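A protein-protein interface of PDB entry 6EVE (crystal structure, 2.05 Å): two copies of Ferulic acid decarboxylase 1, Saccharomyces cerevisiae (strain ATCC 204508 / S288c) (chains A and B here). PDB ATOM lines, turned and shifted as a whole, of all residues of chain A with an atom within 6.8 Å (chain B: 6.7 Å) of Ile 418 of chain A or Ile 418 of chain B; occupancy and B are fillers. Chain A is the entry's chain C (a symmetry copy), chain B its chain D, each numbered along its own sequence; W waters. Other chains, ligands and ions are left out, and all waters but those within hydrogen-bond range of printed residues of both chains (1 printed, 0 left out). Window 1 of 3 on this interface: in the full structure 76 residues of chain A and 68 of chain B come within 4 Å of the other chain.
Water W1 lies within hydrogen-bond range of OH of Tyr 421 of chain A and OH of Tyr 421 of chain B.
Printed residues of chain B within 4 Å of Ala 358 of chain A: Val 422.
Phe 414 of chain A touches none of the printed residues of chain B.
Printed residues of chain B within 4 Å of Ile 418 of chain A: Ile 418 (3.97 Å).
Of the printed residues of chain B, Trp 419 of chain A touches Gln 359.
Of the printed residues of chain A, Gln 359 of chain B touches Trp 419.
Of the printed residues of chain A, Ile 418 of chain B touches Ile 418.
The nearest residue of chain A that does not touch Ile 418 of chain B is Phe 414 of chain A (4.2 Å).
Trp 362 of chain A touches Val 422 of chain B, and with the chains exchanged Val 422 of chain A touches Trp 362 of chain B.
Ile 418 of chain B touches its own counterpart, Ile 418 of chain A.
Trp 419 of chain A touches Gln 359 of chain B, but with the chains exchanged Gln 359 of chain A does not touch Trp 419 of chain B (4.01 Å).
Tyr 421 of chain A touches its own counterpart, Tyr 421 of chain B.
Of the 7 pairs that touch across the chains among the printed residues, 6 have their exchanged pair printed and touching as well.
Printed residues of chain B that touch a printed residue of chain A: Ala 358, Gln 359, Trp 362, Ile 418, Tyr 421 and Val 422.
Printed residues of chain A that touch a printed residue of chain B: Ala 358, Trp 362, Ile 418, Trp 419, Tyr 421 and Val 422.
Hydrophobic or aromatic side chains of chain A within 4 Å of the printed part of chain B: Trp 362, Ile 418, Trp 419, Tyr 421 and Val 422.
Among the printed residues, 7 pairs touch across the chains.
O of Trp 419 of chain A sits at hydrogen-bond distance from OG1 of Thr 423 of chain A, at 2.6 Å.
Among the printed residues, merely in contact across the chains: Ala 358 of chain A with Val 422 of chain B, Trp 362 of chain A with Val 422 of chain B, Ile 418 of chain A with Ile 418 of chain B, Trp 419 of chain A with Gln 359 of chain B, Tyr 421 of chain A with Tyr 421 of chain B, Val 422 of chain A with Ala 358 of chain B and Val 422 of chain A with Trp 362 of chain B.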
ATOM      1  N   GLU A 357       6.681 -17.331 -21.731  1.00  0.00           N
ATOM      2  CA  GLU A 357       5.781 -16.461 -20.968  1.00  0.00           C
ATOM      3  C   GLU A 357       5.936 -15.010 -21.396  1.00  0.00           C
ATOM      4  O   GLU A 357       4.959 -14.266 -21.312  1.00  0.00           O
ATOM      5  CB  GLU A 357       6.033 -16.595 -19.455  1.00  0.00           C
ATOM      6  CG  GLU A 357       5.788 -18.011 -18.908  1.00  0.00           C
ATOM      7  CD  GLU A 357       6.993 -18.962 -18.951  1.00  0.00           C
ATOM      8  OE1 GLU A 357       7.999 -18.695 -19.656  1.00  0.00           O
ATOM      9  OE2 GLU A 357       6.961 -20.026 -18.271  1.00  0.00           O
ATOM     10  N   ALA A 358       7.126 -14.596 -21.873  1.00  0.00           N
ATOM     11  CA  ALA A 358       7.327 -13.218 -22.382  1.00  0.00           C
ATOM     12  C   ALA A 358       7.018 -13.026 -23.894  1.00  0.00           C
ATOM     13  O   ALA A 358       7.343 -11.964 -24.461  1.00  0.00           O
ATOM     14  CB  ALA A 358       8.732 -12.715 -22.061  1.00  0.00           C
ATOM     15  N   GLN A 359       6.375 -14.035 -24.497  1.00  0.00           N
ATOM     16  CA  GLN A 359       5.846 -13.998 -25.869  1.00  0.00           C
ATOM     17  C   GLN A 359       6.955 -13.677 -26.880  1.00  0.00           C
ATOM     18  O   GLN A 359       6.730 -12.933 -27.836  1.00  0.00           O
ATOM     19  CB  GLN A 359       4.669 -13.019 -26.027  1.00  0.00           C
ATOM     20  CG  GLN A 359       3.440 -13.311 -25.167  1.00  0.00           C
ATOM     21  CD  GLN A 359       2.630 -14.536 -25.560  1.00  0.00           C
ATOM     22  OE1 GLN A 359       2.440 -14.886 -26.783  1.00  0.00           O
ATOM     23  NE2 GLN A 359       2.080 -15.168 -24.538  1.00  0.00           N
ATOM     24  N   TRP A 362      11.498 -10.946 -24.857  1.00  0.00           N
ATOM     25  CA  TRP A 362      12.572 -10.857 -23.874  1.00  0.00           C
ATOM     26  C   TRP A 362      13.632 -11.897 -24.294  1.00  0.00           C
ATOM     27  O   TRP A 362      13.302 -13.077 -24.454  1.00  0.00           O
ATOM     28  CB  TRP A 362      12.082 -11.258 -22.435  1.00  0.00           C
ATOM     29  CG  TRP A 362      11.326 -10.241 -21.630  1.00  0.00           C
ATOM     30  CD1 TRP A 362      10.773  -9.080 -22.068  1.00  0.00           C
ATOM     31  CD2 TRP A 362      11.002 -10.333 -20.228  1.00  0.00           C
ATOM     32  NE1 TRP A 362      10.169  -8.416 -21.021  1.00  0.00           N
ATOM     33  CE2 TRP A 362      10.302  -9.156 -19.881  1.00  0.00           C
ATOM     34  CE3 TRP A 362      11.274 -11.277 -19.238  1.00  0.00           C
ATOM     35  CZ2 TRP A 362       9.857  -8.869 -18.552  1.00  0.00           C
ATOM     36  CZ3 TRP A 362      10.828 -10.997 -17.868  1.00  0.00           C
ATOM     37  CH2 TRP A 362      10.116  -9.803 -17.568  1.00  0.00           C
ATOM     38  N   ILE A 409      21.605 -18.130 -12.110  1.00  0.00           N
ATOM     39  CA  ILE A 409      20.200 -18.216 -12.574  1.00  0.00           C
ATOM     40  C   ILE A 409      20.074 -19.219 -13.737  1.00  0.00           C
ATOM     41  O   ILE A 409      20.784 -19.089 -14.745  1.00  0.00           O
ATOM     42  CB  ILE A 409      19.665 -16.828 -13.075  1.00  0.00           C
ATOM     43  CG1 ILE A 409      19.662 -15.770 -11.964  1.00  0.00           C
ATOM     44  CG2 ILE A 409      18.264 -16.967 -13.681  1.00  0.00           C
ATOM     45  CD1 ILE A 409      18.976 -16.162 -10.671  1.00  0.00           C
ATOM     46  N   ASN A 413      14.336 -21.706 -16.720  1.00  0.00           N
ATOM     47  CA  ASN A 413      13.261 -21.837 -15.756  1.00  0.00           C
ATOM     48  C   ASN A 413      12.661 -20.437 -15.515  1.00  0.00           C
ATOM     49  O   ASN A 413      13.293 -19.595 -14.876  1.00  0.00           O
ATOM     50  CB  ASN A 413      13.916 -22.402 -14.481  1.00  0.00           C
ATOM     51  CG  ASN A 413      12.924 -22.713 -13.369  1.00  0.00           C
ATOM     52  OD1 ASN A 413      11.741 -22.414 -13.431  1.00  0.00           O
ATOM     53  ND2 ASN A 413      13.453 -23.297 -12.309  1.00  0.00           N
ATOM     54  N   PHE A 414      11.449 -20.192 -15.955  1.00  0.00           N
ATOM     55  CA  PHE A 414      10.899 -18.855 -15.779  1.00  0.00           C
ATOM     56  C   PHE A 414      10.687 -18.365 -14.323  1.00  0.00           C
ATOM     57  O   PHE A 414      10.573 -17.145 -14.084  1.00  0.00           O
ATOM     58  CB  PHE A 414       9.598 -18.668 -16.528  1.00  0.00           C
ATOM     59  CG  PHE A 414       9.221 -17.208 -16.703  1.00  0.00           C
ATOM     60  CD1 PHE A 414      10.072 -16.334 -17.417  1.00  0.00           C
ATOM     61  CD2 PHE A 414       8.031 -16.705 -16.173  1.00  0.00           C
ATOM     62  CE1 PHE A 414       9.743 -14.985 -17.592  1.00  0.00           C
ATOM     63  CE2 PHE A 414       7.708 -15.354 -16.329  1.00  0.00           C
ATOM     64  CZ  PHE A 414       8.566 -14.499 -17.051  1.00  0.00           C
ATOM     65  N   LYS A 415      10.625 -19.281 -13.372  1.00  0.00           N
ATOM     66  CA  LYS A 415      10.528 -18.855 -11.949  1.00  0.00           C
ATOM     67  C   LYS A 415      11.837 -18.233 -11.497  1.00  0.00           C
ATOM     68  O   LYS A 415      11.837 -17.292 -10.701  1.00  0.00           O
ATOM     69  CB  LYS A 415      10.238 -20.014 -11.016  1.00  0.00           C
ATOM     70  CG  LYS A 415       8.922 -20.747 -11.210  1.00  0.00           C
ATOM     71  CD  LYS A 415       9.007 -22.138 -10.575  1.00  0.00           C
ATOM     72  CE  LYS A 415       7.714 -22.911 -10.774  1.00  0.00           C
ATOM     73  NZ  LYS A 415       6.682 -22.495  -9.772  1.00  0.00           N
ATOM     74  N   GLU A 416      12.957 -18.754 -11.974  1.00  0.00           N
ATOM     75  CA  GLU A 416      14.212 -18.113 -11.619  1.00  0.00           C
ATOM     76  C   GLU A 416      14.389 -16.772 -12.275  1.00  0.00           C
ATOM     77  O   GLU A 416      14.936 -15.887 -11.657  1.00  0.00           O
ATOM     78  CB  GLU A 416      15.405 -19.025 -11.831  1.00  0.00           C
ATOM     79  CG  GLU A 416      15.360 -20.126 -10.777  1.00  0.00           C
ATOM     80  CD  GLU A 416      16.595 -21.014 -10.738  1.00  0.00           C
ATOM     81  OE1 GLU A 416      17.741 -20.541 -10.929  1.00  0.00           O
ATOM     82  OE2 GLU A 416      16.398 -22.209 -10.486  1.00  0.00           O
ATOM     83  N   VAL A 417      13.887 -16.629 -13.517  1.00  0.00           N
ATOM     84  CA  VAL A 417      14.064 -15.435 -14.315  1.00  0.00           C
ATOM     85  C   VAL A 417      13.190 -14.325 -13.731  1.00  0.00           C
ATOM     86  O   VAL A 417      13.618 -13.202 -13.650  1.00  0.00           O
ATOM     87  CB  VAL A 417      13.694 -15.685 -15.822  1.00  0.00           C
ATOM     88  CG1 VAL A 417      13.735 -14.413 -16.610  1.00  0.00           C
ATOM     89  CG2 VAL A 417      14.643 -16.664 -16.481  1.00  0.00           C
ATOM     90  N   ILE A 418      11.931 -14.591 -13.359  1.00  0.00           N
ATOM     91  CA  ILE A 418      11.114 -13.474 -12.864  1.00  0.00           C
ATOM     92  C   ILE A 418      11.644 -12.997 -11.489  1.00  0.00           C
ATOM     93  O   ILE A 418      11.720 -11.812 -11.245  1.00  0.00           O
ATOM     94  CB  ILE A 418       9.584 -13.752 -12.933  1.00  0.00           C
ATOM     95  CG1 ILE A 418       8.796 -12.492 -12.574  1.00  0.00           C
ATOM     96  CG2 ILE A 418       9.195 -14.870 -11.992  1.00  0.00           C
ATOM     97  CD1 ILE A 418       8.768 -11.429 -13.650  1.00  0.00           C
ATOM     98  N   TRP A 419      12.083 -13.925 -10.655  1.00  0.00           N
ATOM     99  CA  TRP A 419      12.781 -13.581  -9.392  1.00  0.00           C
ATOM    100  C   TRP A 419      13.979 -12.634  -9.568  1.00  0.00           C
ATOM    101  O   TRP A 419      14.066 -11.566  -8.900  1.00  0.00           O
ATOM    102  CB  TRP A 419      13.231 -14.845  -8.662  1.00  0.00           C
ATOM    103  CG  TRP A 419      13.960 -14.596  -7.349  1.00  0.00           C
ATOM    104  CD1 TRP A 419      13.499 -13.893  -6.259  1.00  0.00           C
ATOM    105  CD2 TRP A 419      15.248 -15.030  -7.031  1.00  0.00           C
ATOM    106  NE1 TRP A 419      14.463 -13.862  -5.279  1.00  0.00           N
ATOM    107  CE2 TRP A 419      15.537 -14.580  -5.720  1.00  0.00           C
ATOM    108  CE3 TRP A 419      16.209 -15.776  -7.723  1.00  0.00           C
ATOM    109  CZ2 TRP A 419      16.741 -14.865  -5.072  1.00  0.00           C
ATOM    110  CZ3 TRP A 419      17.418 -16.065  -7.092  1.00  0.00           C
ATOM    111  CH2 TRP A 419      17.668 -15.619  -5.755  1.00  0.00           C
ATOM    112  N   ALA A 420      14.886 -12.991 -10.462  1.00  0.00           N
ATOM    113  CA  ALA A 420      16.070 -12.127 -10.731  1.00  0.00           C
ATOM    114  C   ALA A 420      15.616 -10.803 -11.313  1.00  0.00           C
ATOM    115  O   ALA A 420      16.156  -9.812 -10.929  1.00  0.00           O
ATOM    116  CB  ALA A 420      17.071 -12.802 -11.661  1.00  0.00           C
ATOM    117  N   TYR A 421      14.602 -10.780 -12.204  1.00  0.00           N
ATOM    118  CA  TYR A 421      14.177  -9.543 -12.838  1.00  0.00           C
ATOM    119  C   TYR A 421      13.650  -8.511 -11.792  1.00  0.00           C
ATOM    120  O   TYR A 421      14.157  -7.415 -11.702  1.00  0.00           O
ATOM    121  CB  TYR A 421      13.104  -9.845 -13.881  1.00  0.00           C
ATOM    122  CG  TYR A 421      12.705  -8.667 -14.717  1.00  0.00           C
ATOM    123  CD1 TYR A 421      13.504  -8.244 -15.810  1.00  0.00           C
ATOM    124  CD2 TYR A 421      11.551  -7.937 -14.427  1.00  0.00           C
ATOM    125  CE1 TYR A 421      13.135  -7.151 -16.574  1.00  0.00           C
ATOM    126  CE2 TYR A 421      11.184  -6.841 -15.162  1.00  0.00           C
ATOM    127  CZ  TYR A 421      11.968  -6.455 -16.256  1.00  0.00           C
ATOM    128  OH  TYR A 421      11.581  -5.356 -17.013  1.00  0.00           O
ATOM    129  N   VAL A 422      12.647  -8.879 -11.000  1.00  0.00           N
ATOM    130  CA  VAL A 422      12.063  -7.940 -10.016  1.00  0.00           C
ATOM    131  C   VAL A 422      12.978  -7.611  -8.844  1.00  0.00           C
ATOM    132  O   VAL A 422      12.905  -6.494  -8.339  1.00  0.00           O
ATOM    133  CB  VAL A 422      10.694  -8.380  -9.462  1.00  0.00           C
ATOM    134  CG1 VAL A 422       9.778  -8.744 -10.619  1.00  0.00           C
ATOM    135  CG2 VAL A 422      10.856  -9.568  -8.536  1.00  0.00           C
ATOM    136  N   THR A 423      13.853  -8.518  -8.419  1.00  0.00           N
ATOM    137  CA  THR A 423      14.705  -8.256  -7.216  1.00  0.00           C
ATOM    138  C   THR A 423      16.129  -7.670  -7.494  1.00  0.00           C
ATOM    139  O   THR A 423      16.813  -7.195  -6.556  1.00  0.00           O
ATOM    140  CB  THR A 423      14.875  -9.498  -6.331  1.00  0.00           C
ATOM    141  OG1 THR A 423      15.596 -10.539  -7.003  1.00  0.00           O
ATOM    142  CG2 THR A 423      13.562 -10.011  -5.901  1.00  0.00           C
ATOM    143  N   GLU B 357       4.639 -13.908  -7.109  1.00  0.00           N
ATOM    144  CA  GLU B 357       5.791 -14.153  -7.989  1.00  0.00           C
ATOM    145  C   GLU B 357       6.780 -12.994  -8.037  1.00  0.00           C
ATOM    146  O   GLU B 357       7.985 -13.215  -8.206  1.00  0.00           O
ATOM    147  CB  GLU B 357       5.301 -14.452  -9.428  1.00  0.00           C
ATOM    148  CG  GLU B 357       4.547 -15.787  -9.574  1.00  0.00           C
ATOM    149  CD  GLU B 357       3.037 -15.740  -9.291  1.00  0.00           C
ATOM    150  OE1 GLU B 357       2.479 -14.757  -8.752  1.00  0.00           O
ATOM    151  OE2 GLU B 357       2.377 -16.742  -9.597  1.00  0.00           O
ATOM    152  N   ALA B 358       6.255 -11.767  -7.915  1.00  0.00           N
ATOM    153  CA  ALA B 358       7.053 -10.549  -7.797  1.00  0.00           C
ATOM    154  C   ALA B 358       7.485 -10.118  -6.371  1.00  0.00           C
ATOM    155  O   ALA B 358       7.905  -8.973  -6.205  1.00  0.00           O
ATOM    156  CB  ALA B 358       6.351  -9.381  -8.497  1.00  0.00           C
ATOM    157  N   GLN B 359       7.436 -11.025  -5.404  1.00  0.00           N
ATOM    158  CA  GLN B 359       7.998 -10.866  -4.071  1.00  0.00           C
ATOM    159  C   GLN B 359       7.545  -9.592  -3.367  1.00  0.00           C
ATOM    160  O   GLN B 359       8.353  -8.950  -2.659  1.00  0.00           O
ATOM    161  CB  GLN B 359       9.530 -10.908  -4.154  1.00  0.00           C
ATOM    162  CG  GLN B 359      10.102 -12.133  -4.854  1.00  0.00           C
ATOM    163  CD  GLN B 359      10.081 -13.407  -4.020  1.00  0.00           C
ATOM    164  OE1 GLN B 359      10.158 -13.416  -2.745  1.00  0.00           O
ATOM    165  NE2 GLN B 359       9.982 -14.493  -4.714  1.00  0.00           N
ATOM    166  N   TRP B 362       5.672  -5.468  -6.667  1.00  0.00           N
ATOM    167  CA  TRP B 362       4.734  -5.030  -7.708  1.00  0.00           C
ATOM    168  C   TRP B 362       3.312  -4.865  -7.182  1.00  0.00           C
ATOM    169  O   TRP B 362       2.778  -5.782  -6.557  1.00  0.00           O
ATOM    170  CB  TRP B 362       4.688  -6.077  -8.863  1.00  0.00           C
ATOM    171  CG  TRP B 362       5.859  -6.029  -9.895  1.00  0.00           C
ATOM    172  CD1 TRP B 362       7.034  -5.345  -9.795  1.00  0.00           C
ATOM    173  CD2 TRP B 362       5.905  -6.714 -11.152  1.00  0.00           C
ATOM    174  NE1 TRP B 362       7.819  -5.555 -10.949  1.00  0.00           N
ATOM    175  CE2 TRP B 362       7.132  -6.383 -11.784  1.00  0.00           C
ATOM    176  CE3 TRP B 362       5.023  -7.552 -11.811  1.00  0.00           C
ATOM    177  CZ2 TRP B 362       7.473  -6.859 -13.060  1.00  0.00           C
ATOM    178  CZ3 TRP B 362       5.368  -8.063 -13.049  1.00  0.00           C
ATOM    179  CH2 TRP B 362       6.579  -7.714 -13.673  1.00  0.00           C
ATOM    180  N   ASN B 413      -4.524 -13.584 -11.420  1.00  0.00           N
ATOM    181  CA  ASN B 413      -3.913 -14.684 -12.141  1.00  0.00           C
ATOM    182  C   ASN B 413      -2.575 -14.182 -12.798  1.00  0.00           C
ATOM    183  O   ASN B 413      -2.586 -13.383 -13.748  1.00  0.00           O
ATOM    184  CB  ASN B 413      -4.938 -15.093 -13.210  1.00  0.00           C
ATOM    185  CG  ASN B 413      -4.439 -16.211 -14.137  1.00  0.00           C
ATOM    186  OD1 ASN B 413      -3.258 -16.609 -14.096  1.00  0.00           O
ATOM    187  ND2 ASN B 413      -5.365 -16.768 -14.941  1.00  0.00           N
ATOM    188  N   PHE B 414      -1.435 -14.681 -12.353  1.00  0.00           N
ATOM    189  CA  PHE B 414      -0.152 -14.146 -12.823  1.00  0.00           C
ATOM    190  C   PHE B 414       0.104 -14.437 -14.310  1.00  0.00           C
ATOM    191  O   PHE B 414       0.894 -13.734 -14.960  1.00  0.00           O
ATOM    192  CB  PHE B 414       1.037 -14.620 -11.945  1.00  0.00           C
ATOM    193  CG  PHE B 414       2.302 -13.787 -12.132  1.00  0.00           C
ATOM    194  CD1 PHE B 414       2.296 -12.406 -11.859  1.00  0.00           C
ATOM    195  CD2 PHE B 414       3.458 -14.362 -12.662  1.00  0.00           C
ATOM    196  CE1 PHE B 414       3.443 -11.642 -12.072  1.00  0.00           C
ATOM    197  CE2 PHE B 414       4.609 -13.605 -12.848  1.00  0.00           C
ATOM    198  CZ  PHE B 414       4.612 -12.254 -12.545  1.00  0.00           C
ATOM    199  N   LYS B 415      -0.567 -15.440 -14.865  1.00  0.00           N
ATOM    200  CA  LYS B 415      -0.492 -15.644 -16.315  1.00  0.00           C
ATOM    201  C   LYS B 415      -0.953 -14.426 -17.133  1.00  0.00           C
ATOM    202  O   LYS B 415      -0.302 -14.083 -18.140  1.00  0.00           O
ATOM    203  CB  LYS B 415      -1.215 -16.914 -16.754  1.00  0.00           C
ATOM    204  CG  LYS B 415      -0.502 -18.164 -16.277  1.00  0.00           C
ATOM    205  CD  LYS B 415      -1.319 -19.403 -16.577  1.00  0.00           C
ATOM    206  CE  LYS B 415      -0.784 -20.530 -15.709  1.00  0.00           C
ATOM    207  NZ  LYS B 415      -1.375 -21.858 -16.046  1.00  0.00           N
ATOM    208  N   GLU B 416      -2.042 -13.781 -16.715  1.00  0.00           N
ATOM    209  CA  GLU B 416      -2.579 -12.679 -17.444  1.00  0.00           C
ATOM    210  C   GLU B 416      -1.823 -11.407 -17.108  1.00  0.00           C
ATOM    211  O   GLU B 416      -1.690 -10.528 -17.978  1.00  0.00           O
ATOM    212  CB  GLU B 416      -4.090 -12.492 -17.174  1.00  0.00           C
ATOM    213  CG  GLU B 416      -4.938 -13.716 -17.590  1.00  0.00           C
ATOM    214  CD  GLU B 416      -6.460 -13.478 -17.648  1.00  0.00           C
ATOM    215  OE1 GLU B 416      -6.967 -12.309 -17.722  1.00  0.00           O
ATOM    216  OE2 GLU B 416      -7.162 -14.512 -17.613  1.00  0.00           O
ATOM    217  N   VAL B 417      -1.328 -11.281 -15.867  1.00  0.00           N
ATOM    218  CA  VAL B 417      -0.517 -10.144 -15.516  1.00  0.00           C
ATOM    219  C   VAL B 417       0.755 -10.043 -16.379  1.00  0.00           C
ATOM    220  O   VAL B 417       1.022  -8.980 -16.906  1.00  0.00           O
ATOM    221  CB  VAL B 417      -0.162 -10.070 -13.993  1.00  0.00           C
ATOM    222  CG1 VAL B 417       0.833  -8.938 -13.682  1.00  0.00           C
ATOM    223  CG2 VAL B 417      -1.439  -9.823 -13.185  1.00  0.00           C
ATOM    224  N   ILE B 418       1.571 -11.093 -16.458  1.00  0.00           N
ATOM    225  CA  ILE B 418       2.836 -11.010 -17.192  1.00  0.00           C
ATOM    226  C   ILE B 418       2.603 -10.825 -18.708  1.00  0.00           C
ATOM    227  O   ILE B 418       3.437 -10.165 -19.399  1.00  0.00           O
ATOM    228  CB  ILE B 418       3.752 -12.201 -16.872  1.00  0.00           C
ATOM    229  CG1 ILE B 418       5.204 -11.942 -17.356  1.00  0.00           C
ATOM    230  CG2 ILE B 418       3.222 -13.491 -17.494  1.00  0.00           C
ATOM    231  CD1 ILE B 418       5.997 -11.005 -16.466  1.00  0.00           C
ATOM    232  N   TRP B 419       1.471 -11.369 -19.213  1.00  0.00           N
ATOM    233  CA  TRP B 419       1.040 -11.205 -20.611  1.00  0.00           C
ATOM    234  C   TRP B 419       0.795  -9.725 -20.959  1.00  0.00           C
ATOM    235  O   TRP B 419       1.326  -9.192 -21.975  1.00  0.00           O
ATOM    236  CB  TRP B 419      -0.194 -12.037 -20.925  1.00  0.00           C
ATOM    237  CG  TRP B 419      -0.745 -11.784 -22.338  1.00  0.00           C
ATOM    238  CD1 TRP B 419      -0.068 -11.941 -23.513  1.00  0.00           C
ATOM    239  CD2 TRP B 419      -2.059 -11.329 -22.689  1.00  0.00           C
ATOM    240  NE1 TRP B 419      -0.884 -11.619 -24.574  1.00  0.00           N
ATOM    241  CE2 TRP B 419      -2.114 -11.258 -24.098  1.00  0.00           C
ATOM    242  CE3 TRP B 419      -3.210 -10.992 -21.942  1.00  0.00           C
ATOM    243  CZ2 TRP B 419      -3.254 -10.865 -24.782  1.00  0.00           C
ATOM    244  CZ3 TRP B 419      -4.358 -10.612 -22.614  1.00  0.00           C
ATOM    245  CH2 TRP B 419      -4.373 -10.550 -24.043  1.00  0.00           C
ATOM    246  N   ALA B 420       0.060  -9.060 -20.066  1.00  0.00           N
ATOM    247  CA  ALA B 420      -0.270  -7.633 -20.209  1.00  0.00           C
ATOM    248  C   ALA B 420       0.965  -6.725 -20.064  1.00  0.00           C
ATOM    249  O   ALA B 420       1.137  -5.712 -20.766  1.00  0.00           O
ATOM    250  CB  ALA B 420      -1.342  -7.243 -19.194  1.00  0.00           C
ATOM    251  N   TYR B 421       1.809  -7.105 -19.123  1.00  0.00           N
ATOM    252  CA  TYR B 421       2.994  -6.384 -18.827  1.00  0.00           C
ATOM    253  C   TYR B 421       3.923  -6.386 -20.041  1.00  0.00           C
ATOM    254  O   TYR B 421       4.299  -5.312 -20.482  1.00  0.00           O
ATOM    255  CB  TYR B 421       3.673  -6.956 -17.590  1.00  0.00           C
ATOM    256  CG  TYR B 421       4.897  -6.183 -17.147  1.00  0.00           C
ATOM    257  CD1 TYR B 421       4.768  -5.067 -16.330  1.00  0.00           C
ATOM    258  CD2 TYR B 421       6.185  -6.584 -17.508  1.00  0.00           C
ATOM    259  CE1 TYR B 421       5.878  -4.361 -15.888  1.00  0.00           C
ATOM    260  CE2 TYR B 421       7.309  -5.876 -17.064  1.00  0.00           C
ATOM    261  CZ  TYR B 421       7.142  -4.770 -16.249  1.00  0.00           C
ATOM    262  OH  TYR B 421       8.200  -4.061 -15.782  1.00  0.00           O
ATOM    263  N   VAL B 422       4.310  -7.544 -20.554  1.00  0.00           N
ATOM    264  CA  VAL B 422       5.299  -7.534 -21.631  1.00  0.00           C
ATOM    265  C   VAL B 422       4.711  -7.014 -22.977  1.00  0.00           C
ATOM    266  O   VAL B 422       5.462  -6.442 -23.777  1.00  0.00           O
ATOM    267  CB  VAL B 422       6.031  -8.887 -21.847  1.00  0.00           C
ATOM    268  CG1 VAL B 422       6.586  -9.476 -20.564  1.00  0.00           C
ATOM    269  CG2 VAL B 422       5.119  -9.903 -22.482  1.00  0.00           C
ATOM    270  N   THR B 423       3.400  -7.181 -23.213  1.00  0.00           N
ATOM    271  CA  THR B 423       2.831  -6.837 -24.538  1.00  0.00           C
ATOM    272  C   THR B 423       2.239  -5.445 -24.631  1.00  0.00           C
ATOM    273  O   THR B 423       2.040  -4.947 -25.754  1.00  0.00           O
ATOM    274  CB  THR B 423       1.764  -7.852 -25.026  1.00  0.00           C
ATOM    275  OG1 THR B 423       0.594  -7.888 -24.152  1.00  0.00           O
ATOM    276  CG2 THR B 423       2.381  -9.171 -25.118  1.00  0.00           C
HETATM  277  O   HOH W   1      10.636  -2.875 -16.889  1.00  0.00           O
